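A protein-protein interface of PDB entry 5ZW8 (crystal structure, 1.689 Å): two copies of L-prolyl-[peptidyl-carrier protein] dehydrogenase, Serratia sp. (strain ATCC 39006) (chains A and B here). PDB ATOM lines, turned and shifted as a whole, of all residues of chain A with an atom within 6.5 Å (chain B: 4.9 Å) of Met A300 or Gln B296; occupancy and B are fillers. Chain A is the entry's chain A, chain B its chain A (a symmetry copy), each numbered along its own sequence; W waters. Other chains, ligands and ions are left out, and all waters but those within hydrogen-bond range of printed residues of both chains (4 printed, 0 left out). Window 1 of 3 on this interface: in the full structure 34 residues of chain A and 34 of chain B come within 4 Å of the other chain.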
ATOM      1  N   LEU A 292       1.733  -1.405   7.091  1.00  0.00           N
ATOM      2  CA  LEU A 292       3.041  -0.872   6.685  1.00  0.00           C
ATOM      3  C   LEU A 292       4.194  -1.528   7.441  1.00  0.00           C
ATOM      4  O   LEU A 292       5.230  -1.856   6.835  1.00  0.00           O
ATOM      5  CB  LEU A 292       3.081   0.648   6.924  1.00  0.00           C
ATOM      6  CG  LEU A 292       2.167   1.449   5.968  1.00  0.00           C
ATOM      7  CD1 LEU A 292       2.078   2.931   6.461  1.00  0.00           C
ATOM      8  CD2 LEU A 292       2.594   1.397   4.487  1.00  0.00           C
ATOM      9  N   ARG A 293       4.066  -1.630   8.777  1.00  0.00           N
ATOM     10  CA  ARG A 293       5.107  -2.258   9.591  1.00  0.00           C
ATOM     11  C   ARG A 293       5.378  -3.687   9.138  1.00  0.00           C
ATOM     12  O   ARG A 293       6.542  -4.110   9.011  1.00  0.00           O
ATOM     13  CB  ARG A 293       4.720  -2.264  11.077  1.00  0.00           C
ATOM     14  CG  ARG A 293       4.752  -0.822  11.669  1.00  0.00           C
ATOM     15  CD  ARG A 293       4.044  -0.906  13.066  1.00  0.00           C
ATOM     16  NE  ARG A 293       3.884   0.457  13.576  1.00  0.00           N
ATOM     17  CZ  ARG A 293       2.836   0.829  14.318  1.00  0.00           C
ATOM     18  NH1 ARG A 293       1.907  -0.075  14.650  1.00  0.00           N
ATOM     19  NH2 ARG A 293       2.679   2.113  14.668  1.00  0.00           N
ATOM     20  N   GLU A 295       4.798  -5.245   6.349  1.00  0.00           N
ATOM     21  CA  GLU A 295       5.396  -5.436   5.025  1.00  0.00           C
ATOM     22  C   GLU A 295       6.865  -5.029   5.032  1.00  0.00           C
ATOM     23  O   GLU A 295       7.735  -5.747   4.471  1.00  0.00           O
ATOM     24  CB  GLU A 295       4.631  -4.617   3.995  1.00  0.00           C
ATOM     25  CG  GLU A 295       3.124  -5.029   3.836  1.00  0.00           C
ATOM     26  CD  GLU A 295       2.956  -6.536   3.605  1.00  0.00           C
ATOM     27  OE1 GLU A 295       3.767  -7.127   2.861  1.00  0.00           O
ATOM     28  OE2 GLU A 295       2.027  -7.156   4.194  1.00  0.00           O
ATOM     29  N   GLN A 296       7.156  -3.904   5.697  1.00  0.00           N
ATOM     30  CA  GLN A 296       8.543  -3.428   5.758  1.00  0.00           C
ATOM     31  C   GLN A 296       9.451  -4.397   6.511  1.00  0.00           C
ATOM     32  O   GLN A 296      10.550  -4.730   6.044  1.00  0.00           O
ATOM     33  CB  GLN A 296       8.651  -2.085   6.460  1.00  0.00           C
ATOM     34  CG  GLN A 296       8.108  -0.915   5.590  1.00  0.00           C
ATOM     35  CD  GLN A 296       8.097   0.332   6.403  1.00  0.00           C
ATOM     36  OE1 GLN A 296       8.949   1.188   6.218  1.00  0.00           O
ATOM     37  NE2 GLN A 296       7.113   0.469   7.302  1.00  0.00           N
ATOM     38  N   CYS A 297       9.018  -4.844   7.703  1.00  0.00           N
ATOM     39  CA  CYS A 297       9.967  -5.600   8.517  1.00  0.00           C
ATOM     40  C   CYS A 297      10.117  -7.019   8.005  1.00  0.00           C
ATOM     41  O   CYS A 297      11.198  -7.588   8.172  1.00  0.00           O
ATOM     42  CB  CYS A 297       9.575  -5.605   9.997  1.00  0.00           C
ATOM     43  SG  CYS A 297       8.136  -6.548  10.518  1.00  0.00           S
ATOM     44  N   ARG A 298       9.056  -7.576   7.402  1.00  0.00           N
ATOM     45  CA  ARG A 298       9.203  -8.889   6.746  1.00  0.00           C
ATOM     46  C   ARG A 298      10.251  -8.811   5.647  1.00  0.00           C
ATOM     47  O   ARG A 298      11.123  -9.685   5.564  1.00  0.00           O
ATOM     48  CB  ARG A 298       7.869  -9.370   6.159  1.00  0.00           C
ATOM     49  CG  ARG A 298       8.037 -10.762   5.514  1.00  0.00           C
ATOM     50  CD  ARG A 298       6.723 -11.283   4.872  1.00  0.00           C
ATOM     51  NE  ARG A 298       5.754 -11.791   5.843  1.00  0.00           N
ATOM     52  CZ  ARG A 298       4.503 -11.378   5.948  1.00  0.00           C
ATOM     53  NH1 ARG A 298       4.030 -10.420   5.140  1.00  0.00           N
ATOM     54  NH2 ARG A 298       3.721 -11.946   6.864  1.00  0.00           N
ATOM     55  N   LEU A 299      10.205  -7.750   4.817  1.00  0.00           N
ATOM     56  CA  LEU A 299      11.232  -7.641   3.776  1.00  0.00           C
ATOM     57  C   LEU A 299      12.647  -7.481   4.358  1.00  0.00           C
ATOM     58  O   LEU A 299      13.639  -8.065   3.835  1.00  0.00           O
ATOM     59  CB  LEU A 299      10.898  -6.459   2.873  1.00  0.00           C
ATOM     60  CG  LEU A 299       9.713  -6.721   1.923  1.00  0.00           C
ATOM     61  CD1 LEU A 299       9.347  -5.451   1.190  1.00  0.00           C
ATOM     62  CD2 LEU A 299      10.028  -7.802   0.872  1.00  0.00           C
ATOM     63  N   MET A 300      12.797  -6.647   5.412  1.00  0.00           N
ATOM     64  CA  MET A 300      14.115  -6.507   6.023  1.00  0.00           C
ATOM     65  C   MET A 300      14.650  -7.851   6.544  1.00  0.00           C
ATOM     66  O   MET A 300      15.844  -8.170   6.343  1.00  0.00           O
ATOM     67  CB  MET A 300      14.093  -5.483   7.164  1.00  0.00           C
ATOM     68  CG  MET A 300      13.756  -4.048   6.686  1.00  0.00           C
ATOM     69  SD  MET A 300      15.232  -3.329   5.854  1.00  0.00           S
ATOM     70  CE  MET A 300      16.289  -3.035   7.297  1.00  0.00           C
ATOM     71  N   LEU A 301      13.793  -8.644   7.214  1.00  0.00           N
ATOM     72  CA  LEU A 301      14.220  -9.938   7.741  1.00  0.00           C
ATOM     73  C   LEU A 301      14.636 -10.892   6.610  1.00  0.00           C
ATOM     74  O   LEU A 301      15.680 -11.558   6.697  1.00  0.00           O
ATOM     75  CB  LEU A 301      13.077 -10.563   8.538  1.00  0.00           C
ATOM     76  CG  LEU A 301      13.532 -11.902   9.172  1.00  0.00           C
ATOM     77  CD1 LEU A 301      14.706 -11.648  10.081  1.00  0.00           C
ATOM     78  CD2 LEU A 301      12.416 -12.425   9.971  1.00  0.00           C
ATOM     79  N   TYR A 302      13.804 -10.983   5.571  1.00  0.00           N
ATOM     80  CA  TYR A 302      14.099 -11.894   4.460  1.00  0.00           C
ATOM     81  C   TYR A 302      15.406 -11.506   3.799  1.00  0.00           C
ATOM     82  O   TYR A 302      16.247 -12.376   3.493  1.00  0.00           O
ATOM     83  CB  TYR A 302      12.987 -11.840   3.411  1.00  0.00           C
ATOM     84  CG  TYR A 302      11.684 -12.483   3.836  1.00  0.00           C
ATOM     85  CD1 TYR A 302      11.575 -13.159   5.043  1.00  0.00           C
ATOM     86  CD2 TYR A 302      10.615 -12.503   2.963  1.00  0.00           C
ATOM     87  CE1 TYR A 302      10.367 -13.789   5.421  1.00  0.00           C
ATOM     88  CE2 TYR A 302       9.428 -13.133   3.301  1.00  0.00           C
ATOM     89  CZ  TYR A 302       9.310 -13.782   4.524  1.00  0.00           C
ATOM     90  OH  TYR A 302       8.097 -14.384   4.820  1.00  0.00           O
ATOM     91  N   ARG A 303      15.612 -10.195   3.586  1.00  0.00           N
ATOM     92  CA  ARG A 303      16.870  -9.793   2.970  1.00  0.00           C
ATOM     93  C   ARG A 303      18.050 -10.137   3.872  1.00  0.00           C
ATOM     94  O   ARG A 303      19.083 -10.628   3.374  1.00  0.00           O
ATOM     95  CB  ARG A 303      16.880  -8.309   2.600  1.00  0.00           C
ATOM     96  CG  ARG A 303      18.202  -8.019   1.829  1.00  0.00           C
ATOM     97  CD  ARG A 303      18.218  -6.627   1.312  1.00  0.00           C
ATOM     98  NE  ARG A 303      18.409  -5.703   2.446  1.00  0.00           N
ATOM     99  CZ  ARG A 303      18.551  -4.387   2.268  1.00  0.00           C
ATOM    100  NH1 ARG A 303      18.517  -3.922   1.027  1.00  0.00           N
ATOM    101  NH2 ARG A 303      18.691  -3.535   3.294  1.00  0.00           N
ATOM    102  N   ALA A 304      17.942  -9.904   5.206  1.00  0.00           N
ATOM    103  CA  ALA A 304      19.052 -10.186   6.090  1.00  0.00           C
ATOM    104  C   ALA A 304      19.425 -11.677   6.022  1.00  0.00           C
ATOM    105  O   ALA A 304      20.610 -12.030   5.868  1.00  0.00           O
ATOM    106  CB  ALA A 304      18.717  -9.798   7.529  1.00  0.00           C
ATOM    107  N   CYS A 305      18.404 -12.552   6.061  1.00  0.00           N
ATOM    108  CA  CYS A 305      18.629 -14.006   6.068  1.00  0.00           C
ATOM    109  C   CYS A 305      19.187 -14.457   4.718  1.00  0.00           C
ATOM    110  O   CYS A 305      20.148 -15.232   4.662  1.00  0.00           O
ATOM    111  CB  CYS A 305      17.293 -14.733   6.400  1.00  0.00           C
ATOM    112  SG  CYS A 305      16.843 -14.507   8.142  1.00  0.00           S
ATOM    113  N   ASP A 317      22.329  -6.043   9.011  1.00  0.00           N
ATOM    114  CA  ASP A 317      20.975  -6.234   8.528  1.00  0.00           C
ATOM    115  C   ASP A 317      20.143  -6.970   9.550  1.00  0.00           C
ATOM    116  O   ASP A 317      18.975  -6.655   9.725  1.00  0.00           O
ATOM    117  CB  ASP A 317      20.958  -6.983   7.210  1.00  0.00           C
ATOM    118  CG  ASP A 317      21.700  -6.222   6.112  1.00  0.00           C
ATOM    119  OD1 ASP A 317      21.441  -5.015   5.859  1.00  0.00           O
ATOM    120  OD2 ASP A 317      22.633  -6.819   5.569  1.00  0.00           O
ATOM    121  N   ILE A 318      20.737  -7.945  10.236  1.00  0.00           N
ATOM    122  CA  ILE A 318      20.047  -8.657  11.300  1.00  0.00           C
ATOM    123  C   ILE A 318      19.767  -7.725  12.482  1.00  0.00           C
ATOM    124  O   ILE A 318      18.682  -7.781  13.060  1.00  0.00           O
ATOM    125  CB  ILE A 318      20.898  -9.862  11.748  1.00  0.00           C
ATOM    126  CG1 ILE A 318      20.828 -10.963  10.670  1.00  0.00           C
ATOM    127  CG2 ILE A 318      20.321 -10.438  13.039  1.00  0.00           C
ATOM    128  CD1 ILE A 318      19.391 -11.506  10.488  1.00  0.00           C
ATOM    129  N   MET A 320      19.350  -4.515  12.353  1.00  0.00           N
ATOM    130  CA  MET A 320      18.246  -3.637  11.907  1.00  0.00           C
ATOM    131  C   MET A 320      16.906  -4.358  11.932  1.00  0.00           C
ATOM    132  O   MET A 320      15.876  -3.785  12.329  1.00  0.00           O
ATOM    133  CB  MET A 320      18.517  -3.095  10.479  1.00  0.00           C
ATOM    134  CG  MET A 320      19.669  -2.110  10.480  1.00  0.00           C
ATOM    135  SD  MET A 320      19.808  -1.341   8.792  1.00  0.00           S
ATOM    136  CE  MET A 320      20.497  -2.629   7.785  1.00  0.00           C
ATOM    137  N   SER A 321      16.900  -5.609  11.485  1.00  0.00           N
ATOM    138  CA  SER A 321      15.675  -6.397  11.461  1.00  0.00           C
ATOM    139  C   SER A 321      15.156  -6.606  12.859  1.00  0.00           C
ATOM    140  O   SER A 321      13.949  -6.477  13.104  1.00  0.00           O
ATOM    141  CB  SER A 321      15.953  -7.737  10.791  1.00  0.00           C
ATOM    142  OG  SER A 321      16.170  -7.450   9.399  1.00  0.00           O
ATOM    143  N   LEU A 324      13.673  -3.349  14.231  1.00  0.00           N
ATOM    144  CA  LEU A 324      12.379  -2.977  13.619  1.00  0.00           C
ATOM    145  C   LEU A 324      11.266  -3.909  14.087  1.00  0.00           C
ATOM    146  O   LEU A 324      10.167  -3.448  14.446  1.00  0.00           O
ATOM    147  CB  LEU A 324      12.486  -3.037  12.082  1.00  0.00           C
ATOM    148  CG  LEU A 324      13.398  -1.900  11.573  1.00  0.00           C
ATOM    149  CD1 LEU A 324      13.613  -2.158  10.044  1.00  0.00           C
ATOM    150  CD2 LEU A 324      12.737  -0.515  11.726  1.00  0.00           C
ATOM    151  N   ILE A 325      11.534  -5.224  14.044  1.00  0.00           N
ATOM    152  CA  ILE A 325      10.488  -6.224  14.284  1.00  0.00           C
ATOM    153  C   ILE A 325       9.970  -6.080  15.695  1.00  0.00           C
ATOM    154  O   ILE A 325       8.753  -6.096  15.915  1.00  0.00           O
ATOM    155  CB  ILE A 325      11.003  -7.649  13.995  1.00  0.00           C
ATOM    156  CG1 ILE A 325      11.071  -7.791  12.453  1.00  0.00           C
ATOM    157  CG2 ILE A 325      10.045  -8.707  14.548  1.00  0.00           C
ATOM    158  CD1 ILE A 325      11.820  -8.939  11.977  1.00  0.00           C
ATOM    159  N   TYR A 328       8.022  -2.767  16.106  1.00  0.00           N
ATOM    160  CA  TYR A 328       6.751  -2.853  15.402  1.00  0.00           C
ATOM    161  C   TYR A 328       5.807  -3.869  16.049  1.00  0.00           C
ATOM    162  O   TYR A 328       4.595  -3.637  16.053  1.00  0.00           O
ATOM    163  CB  TYR A 328       6.968  -3.247  13.951  1.00  0.00           C
ATOM    164  CG  TYR A 328       7.638  -2.240  13.072  1.00  0.00           C
ATOM    165  CD1 TYR A 328       7.832  -0.946  13.501  1.00  0.00           C
ATOM    166  CD2 TYR A 328       8.037  -2.626  11.771  1.00  0.00           C
ATOM    167  CE1 TYR A 328       8.452  -0.016  12.663  1.00  0.00           C
ATOM    168  CE2 TYR A 328       8.627  -1.671  10.892  1.00  0.00           C
ATOM    169  CZ  TYR A 328       8.807  -0.405  11.383  1.00  0.00           C
ATOM    170  OH  TYR A 328       9.416   0.570  10.568  1.00  0.00           O
ATOM    171  N   LEU B 292      17.545   3.125   8.678  1.00  0.00           N
ATOM    172  CA  LEU B 292      16.378   2.232   8.707  1.00  0.00           C
ATOM    173  C   LEU B 292      15.334   2.609   7.657  1.00  0.00           C
ATOM    174  O   LEU B 292      14.775   1.722   6.989  1.00  0.00           O
ATOM    175  CB  LEU B 292      15.728   2.269  10.102  1.00  0.00           C
ATOM    176  CG  LEU B 292      16.587   1.607  11.203  1.00  0.00           C
ATOM    177  CD1 LEU B 292      15.969   1.930  12.603  1.00  0.00           C
ATOM    178  CD2 LEU B 292      16.777   0.086  11.033  1.00  0.00           C
ATOM    179  N   ARG B 293      14.993   3.908   7.578  1.00  0.00           N
ATOM    180  CA  ARG B 293      14.016   4.375   6.595  1.00  0.00           C
ATOM    181  C   ARG B 293      14.443   4.020   5.176  1.00  0.00           C
ATOM    182  O   ARG B 293      13.631   3.545   4.361  1.00  0.00           O
ATOM    183  CB  ARG B 293      13.810   5.893   6.695  1.00  0.00           C
ATOM    184  CG  ARG B 293      13.066   6.271   8.012  1.00  0.00           C
ATOM    185  CD  ARG B 293      13.196   7.827   8.159  1.00  0.00           C
ATOM    186  NE  ARG B 293      12.675   8.204   9.473  1.00  0.00           N
ATOM    187  CZ  ARG B 293      13.180   9.217  10.185  1.00  0.00           C
ATOM    188  NH1 ARG B 293      14.176   9.951   9.674  1.00  0.00           N
ATOM    189  NH2 ARG B 293      12.742   9.453  11.429  1.00  0.00           N
ATOM    190  N   LEU B 294      15.698   4.338   4.848  1.00  0.00           N
ATOM    191  CA  LEU B 294      16.177   4.149   3.489  1.00  0.00           C
ATOM    192  C   LEU B 294      16.069   2.682   3.102  1.00  0.00           C
ATOM    193  O   LEU B 294      15.545   2.345   2.029  1.00  0.00           O
ATOM    194  CB  LEU B 294      17.628   4.665   3.398  1.00  0.00           C
ATOM    195  CG  LEU B 294      18.306   4.352   2.046  1.00  0.00           C
ATOM    196  CD1 LEU B 294      17.468   5.089   0.901  1.00  0.00           C
ATOM    197  CD2 LEU B 294      19.761   4.862   2.054  1.00  0.00           C
ATOM    198  N   GLU B 295      16.502   1.801   4.003  1.00  0.00           N
ATOM    199  CA  GLU B 295      16.536   0.382   3.638  1.00  0.00           C
ATOM    200  C   GLU B 295      15.122  -0.168   3.482  1.00  0.00           C
ATOM    201  O   GLU B 295      14.825  -0.912   2.509  1.00  0.00           O
ATOM    202  CB  GLU B 295      17.288  -0.403   4.704  1.00  0.00           C
ATOM    203  CG  GLU B 295      18.790   0.019   4.874  1.00  0.00           C
ATOM    204  CD  GLU B 295      19.544   0.032   3.538  1.00  0.00           C
ATOM    205  OE1 GLU B 295      19.320  -0.876   2.710  1.00  0.00           O
ATOM    206  OE2 GLU B 295      20.347   0.973   3.286  1.00  0.00           O
ATOM    207  N   GLN B 296      14.237   0.223   4.407  1.00  0.00           N
ATOM    208  CA  GLN B 296      12.851  -0.256   4.343  1.00  0.00           C
ATOM    209  C   GLN B 296      12.129   0.239   3.092  1.00  0.00           C
ATOM    210  O   GLN B 296      11.466  -0.541   2.392  1.00  0.00           O
ATOM    211  CB  GLN B 296      12.036   0.209   5.537  1.00  0.00           C
ATOM    212  CG  GLN B 296      12.416  -0.544   6.845  1.00  0.00           C
ATOM    213  CD  GLN B 296      11.695   0.076   7.990  1.00  0.00           C
ATOM    214  OE1 GLN B 296      10.729  -0.488   8.481  1.00  0.00           O
ATOM    215  NE2 GLN B 296      12.169   1.240   8.456  1.00  0.00           N
ATOM    216  N   CYS B 297      12.225   1.549   2.806  1.00  0.00           N
ATOM    217  CA  CYS B 297      11.371   2.062   1.737  1.00  0.00           C
ATOM    218  C   CYS B 297      11.921   1.693   0.373  1.00  0.00           C
ATOM    219  O   CYS B 297      11.124   1.537  -0.555  1.00  0.00           O
ATOM    220  CB  CYS B 297      11.171   3.577   1.841  1.00  0.00           C
ATOM    221  SG  CYS B 297      12.552   4.668   1.475  1.00  0.00           S
ATOM    222  N   ARG B 298      13.251   1.563   0.256  1.00  0.00           N
ATOM    223  CA  ARG B 298      13.820   1.049  -1.005  1.00  0.00           C
ATOM    224  C   ARG B 298      13.288  -0.347  -1.288  1.00  0.00           C
ATOM    225  O   ARG B 298      12.869  -0.628  -2.417  1.00  0.00           O
ATOM    226  CB  ARG B 298      15.353   1.020  -0.952  1.00  0.00           C
ATOM    227  CG  ARG B 298      15.927   0.518  -2.294  1.00  0.00           C
ATOM    228  CD  ARG B 298      17.478   0.437  -2.284  1.00  0.00           C
ATOM    229  NE  ARG B 298      18.137   1.734  -2.427  1.00  0.00           N
ATOM    230  CZ  ARG B 298      19.036   2.220  -1.589  1.00  0.00           C
ATOM    231  NH1 ARG B 298      19.406   1.524  -0.505  1.00  0.00           N
ATOM    232  NH2 ARG B 298      19.575   3.409  -1.853  1.00  0.00           N
ATOM    233  N   LEU B 299      13.261  -1.223  -0.264  1.00  0.00           N
ATOM    234  CA  LEU B 299      12.716  -2.561  -0.513  1.00  0.00           C
ATOM    235  C   LEU B 299      11.226  -2.530  -0.893  1.00  0.00           C
ATOM    236  O   LEU B 299      10.763  -3.295  -1.786  1.00  0.00           O
ATOM    237  CB  LEU B 299      12.923  -3.419   0.730  1.00  0.00           C
ATOM    238  CG  LEU B 299      14.384  -3.861   0.942  1.00  0.00           C
ATOM    239  CD1 LEU B 299      14.526  -4.559   2.274  1.00  0.00           C
ATOM    240  CD2 LEU B 299      14.871  -4.827  -0.155  1.00  0.00           C
ATOM    241  N   MET B 300      10.422  -1.694  -0.196  1.00  0.00           N
ATOM    242  CA  MET B 300       9.013  -1.599  -0.562  1.00  0.00           C
ATOM    243  C   MET B 300       8.827  -1.149  -2.020  1.00  0.00           C
ATOM    244  O   MET B 300       7.980  -1.716  -2.747  1.00  0.00           O
ATOM    245  CB  MET B 300       8.259  -0.645   0.373  1.00  0.00           C
ATOM    246  CG  MET B 300       8.226  -1.134   1.843  1.00  0.00           C
ATOM    247  SD  MET B 300       7.004  -2.503   1.994  1.00  0.00           S
ATOM    248  CE  MET B 300       5.463  -1.560   1.848  1.00  0.00           C
ATOM    249  N   TYR B 328       9.299   9.483   4.904  1.00  0.00           N
ATOM    250  CA  TYR B 328      10.683   9.279   5.304  1.00  0.00           C
ATOM    251  C   TYR B 328      11.615  10.324   4.687  1.00  0.00           C
ATOM    252  O   TYR B 328      12.580  10.723   5.345  1.00  0.00           O
ATOM    253  CB  TYR B 328      11.162   7.898   4.892  1.00  0.00           C
ATOM    254  CG  TYR B 328      10.553   6.733   5.606  1.00  0.00           C
ATOM    255  CD1 TYR B 328       9.780   6.920   6.730  1.00  0.00           C
ATOM    256  CD2 TYR B 328      10.818   5.427   5.132  1.00  0.00           C
ATOM    257  CE1 TYR B 328       9.226   5.819   7.389  1.00  0.00           C
ATOM    258  CE2 TYR B 328      10.296   4.296   5.827  1.00  0.00           C
ATOM    259  CZ  TYR B 328       9.521   4.548   6.927  1.00  0.00           C
ATOM    260  OH  TYR B 328       8.954   3.468   7.632  1.00  0.00           O
HETATM  261  O   HOH W   1      19.712  -1.318   0.170  1.00  0.00           O
HETATM  262  O   HOH W   2      11.764   2.941  10.828  1.00  0.00           O
HETATM  263  O   HOH W   3       6.006   2.627   8.978  1.00  0.00           O
HETATM  264  O   HOH W   4      17.042  -1.758   0.906  1.00  0.00           O
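Of chain B, only Glu B295 (3.8 Å), Gln B296 (3.8 Å) and Leu B299 (3.9 Å) come within 4 Å of Met A300. Printed residues of chain B within 4 Å of Met A320: Leu B292 (3.7 Å). Of the printed residues of chain A, Glu B295 touches Met A300 and Arg A303. Leu A292 touches none of the printed residues of chain B. Cys A305 touches none of the printed residues of chain B. The nearest printed residue of chain B that does not touch Met A300 is Leu B292 (4.9 Å). The nearest printed residue of chain A that does not touch Leu B292 is Met A300 (4.9 Å).
Water W1 lies within hydrogen-bond range of OE1 of Glu B295 (2.6 Å), NH1 of Arg B298 (2.9 Å) and NH1 of Arg A303 (3.0 Å). Water W4 bridges the guanidinium group of Arg A303 and the backbone carbonyl oxygen of Glu B295. Water W3 bridges the side-chain amide nitrogen (NE2) of Gln A296 (2.9 Å) and the side-chain hydroxyl (OH) of Tyr B328 (3.3 Å). Water W2 bridges NE2 of Gln B296 and OH of Tyr A328.
The backbone carbonyl oxygen (O) of Leu A292 is in hydrogen-bond range of the side-chain amide nitrogen (NE2) of Gln A296, 3.0 Å away. The side-chain amide nitrogen (NE2) of Gln B296 is in hydrogen-bond range of the backbone carbonyl oxygen (O) of Leu B292 (3.0 Å). The side-chain hydroxyl of Ser A321 lies within hydrogen-bond range of the backbone carbonyl oxygen of Met A300. OE2 of Glu A295 lies within salt-bridge range of NH1 of Arg A298 (3.9 Å). OE2 of Glu B295 is in salt-bridge range of NH1 of Arg B298 (3.9 Å).
Among the printed residues, merely in contact across the chains: Leu A324 with Gln B296 (3.6 Å), Met A320 with Leu B292 (3.7 Å), Met A300 with Gln B296 (3.8 Å), Gln A296 with Met B300 (3.8 Å), Glu A295 with Met B300 (3.8 Å), Met A300 with Glu B295 (3.8 Å), Leu A299 with Met B300 (3.9 Å), Met A300 with Leu B299 (3.9 Å), Arg A303 with Leu B299 (3.9 Å), Leu A299 with Leu B299 (3.9 Å) and Leu A324 with Leu B292 (3.96 Å).
Hydrophobic or aromatic side chains of chain B within 4 Å of the printed part of chain A: Leu B292, Leu B299, Met B300 and Tyr B328. Of the 20 printed residues of chain A, 8 touch a printed residue of chain B. Among the printed residues, 15 pairs touch across the chains.
The side-chain amide oxygen of Gln B296 lies close to the side-chain amide oxygen of Gln A296, 3.3 Å away. NH2 of Arg A303 is in salt-bridge range of OE1 of Glu B295, at 2.8 Å. The side-chain amide oxygen (OE1) of Gln B296 sits at hydrogen-bond distance from the side-chain hydroxyl (OH) of Tyr A328. OE1 of Gln A296 sits at hydrogen-bond distance from OH of Tyr B328, 2.7 Å away.
Glu A295 touches Met B300, and with the chains exchanged Met A300 touches Glu B295. Gln B296 touches its own counterpart, Gln A296. Gln A296 touches Tyr B328, and with the chains exchanged Tyr A328 touches Gln B296. Leu A299 touches Met B300, and with the chains exchanged Met A300 touches Leu B299. 9 positions are printed for both chains.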
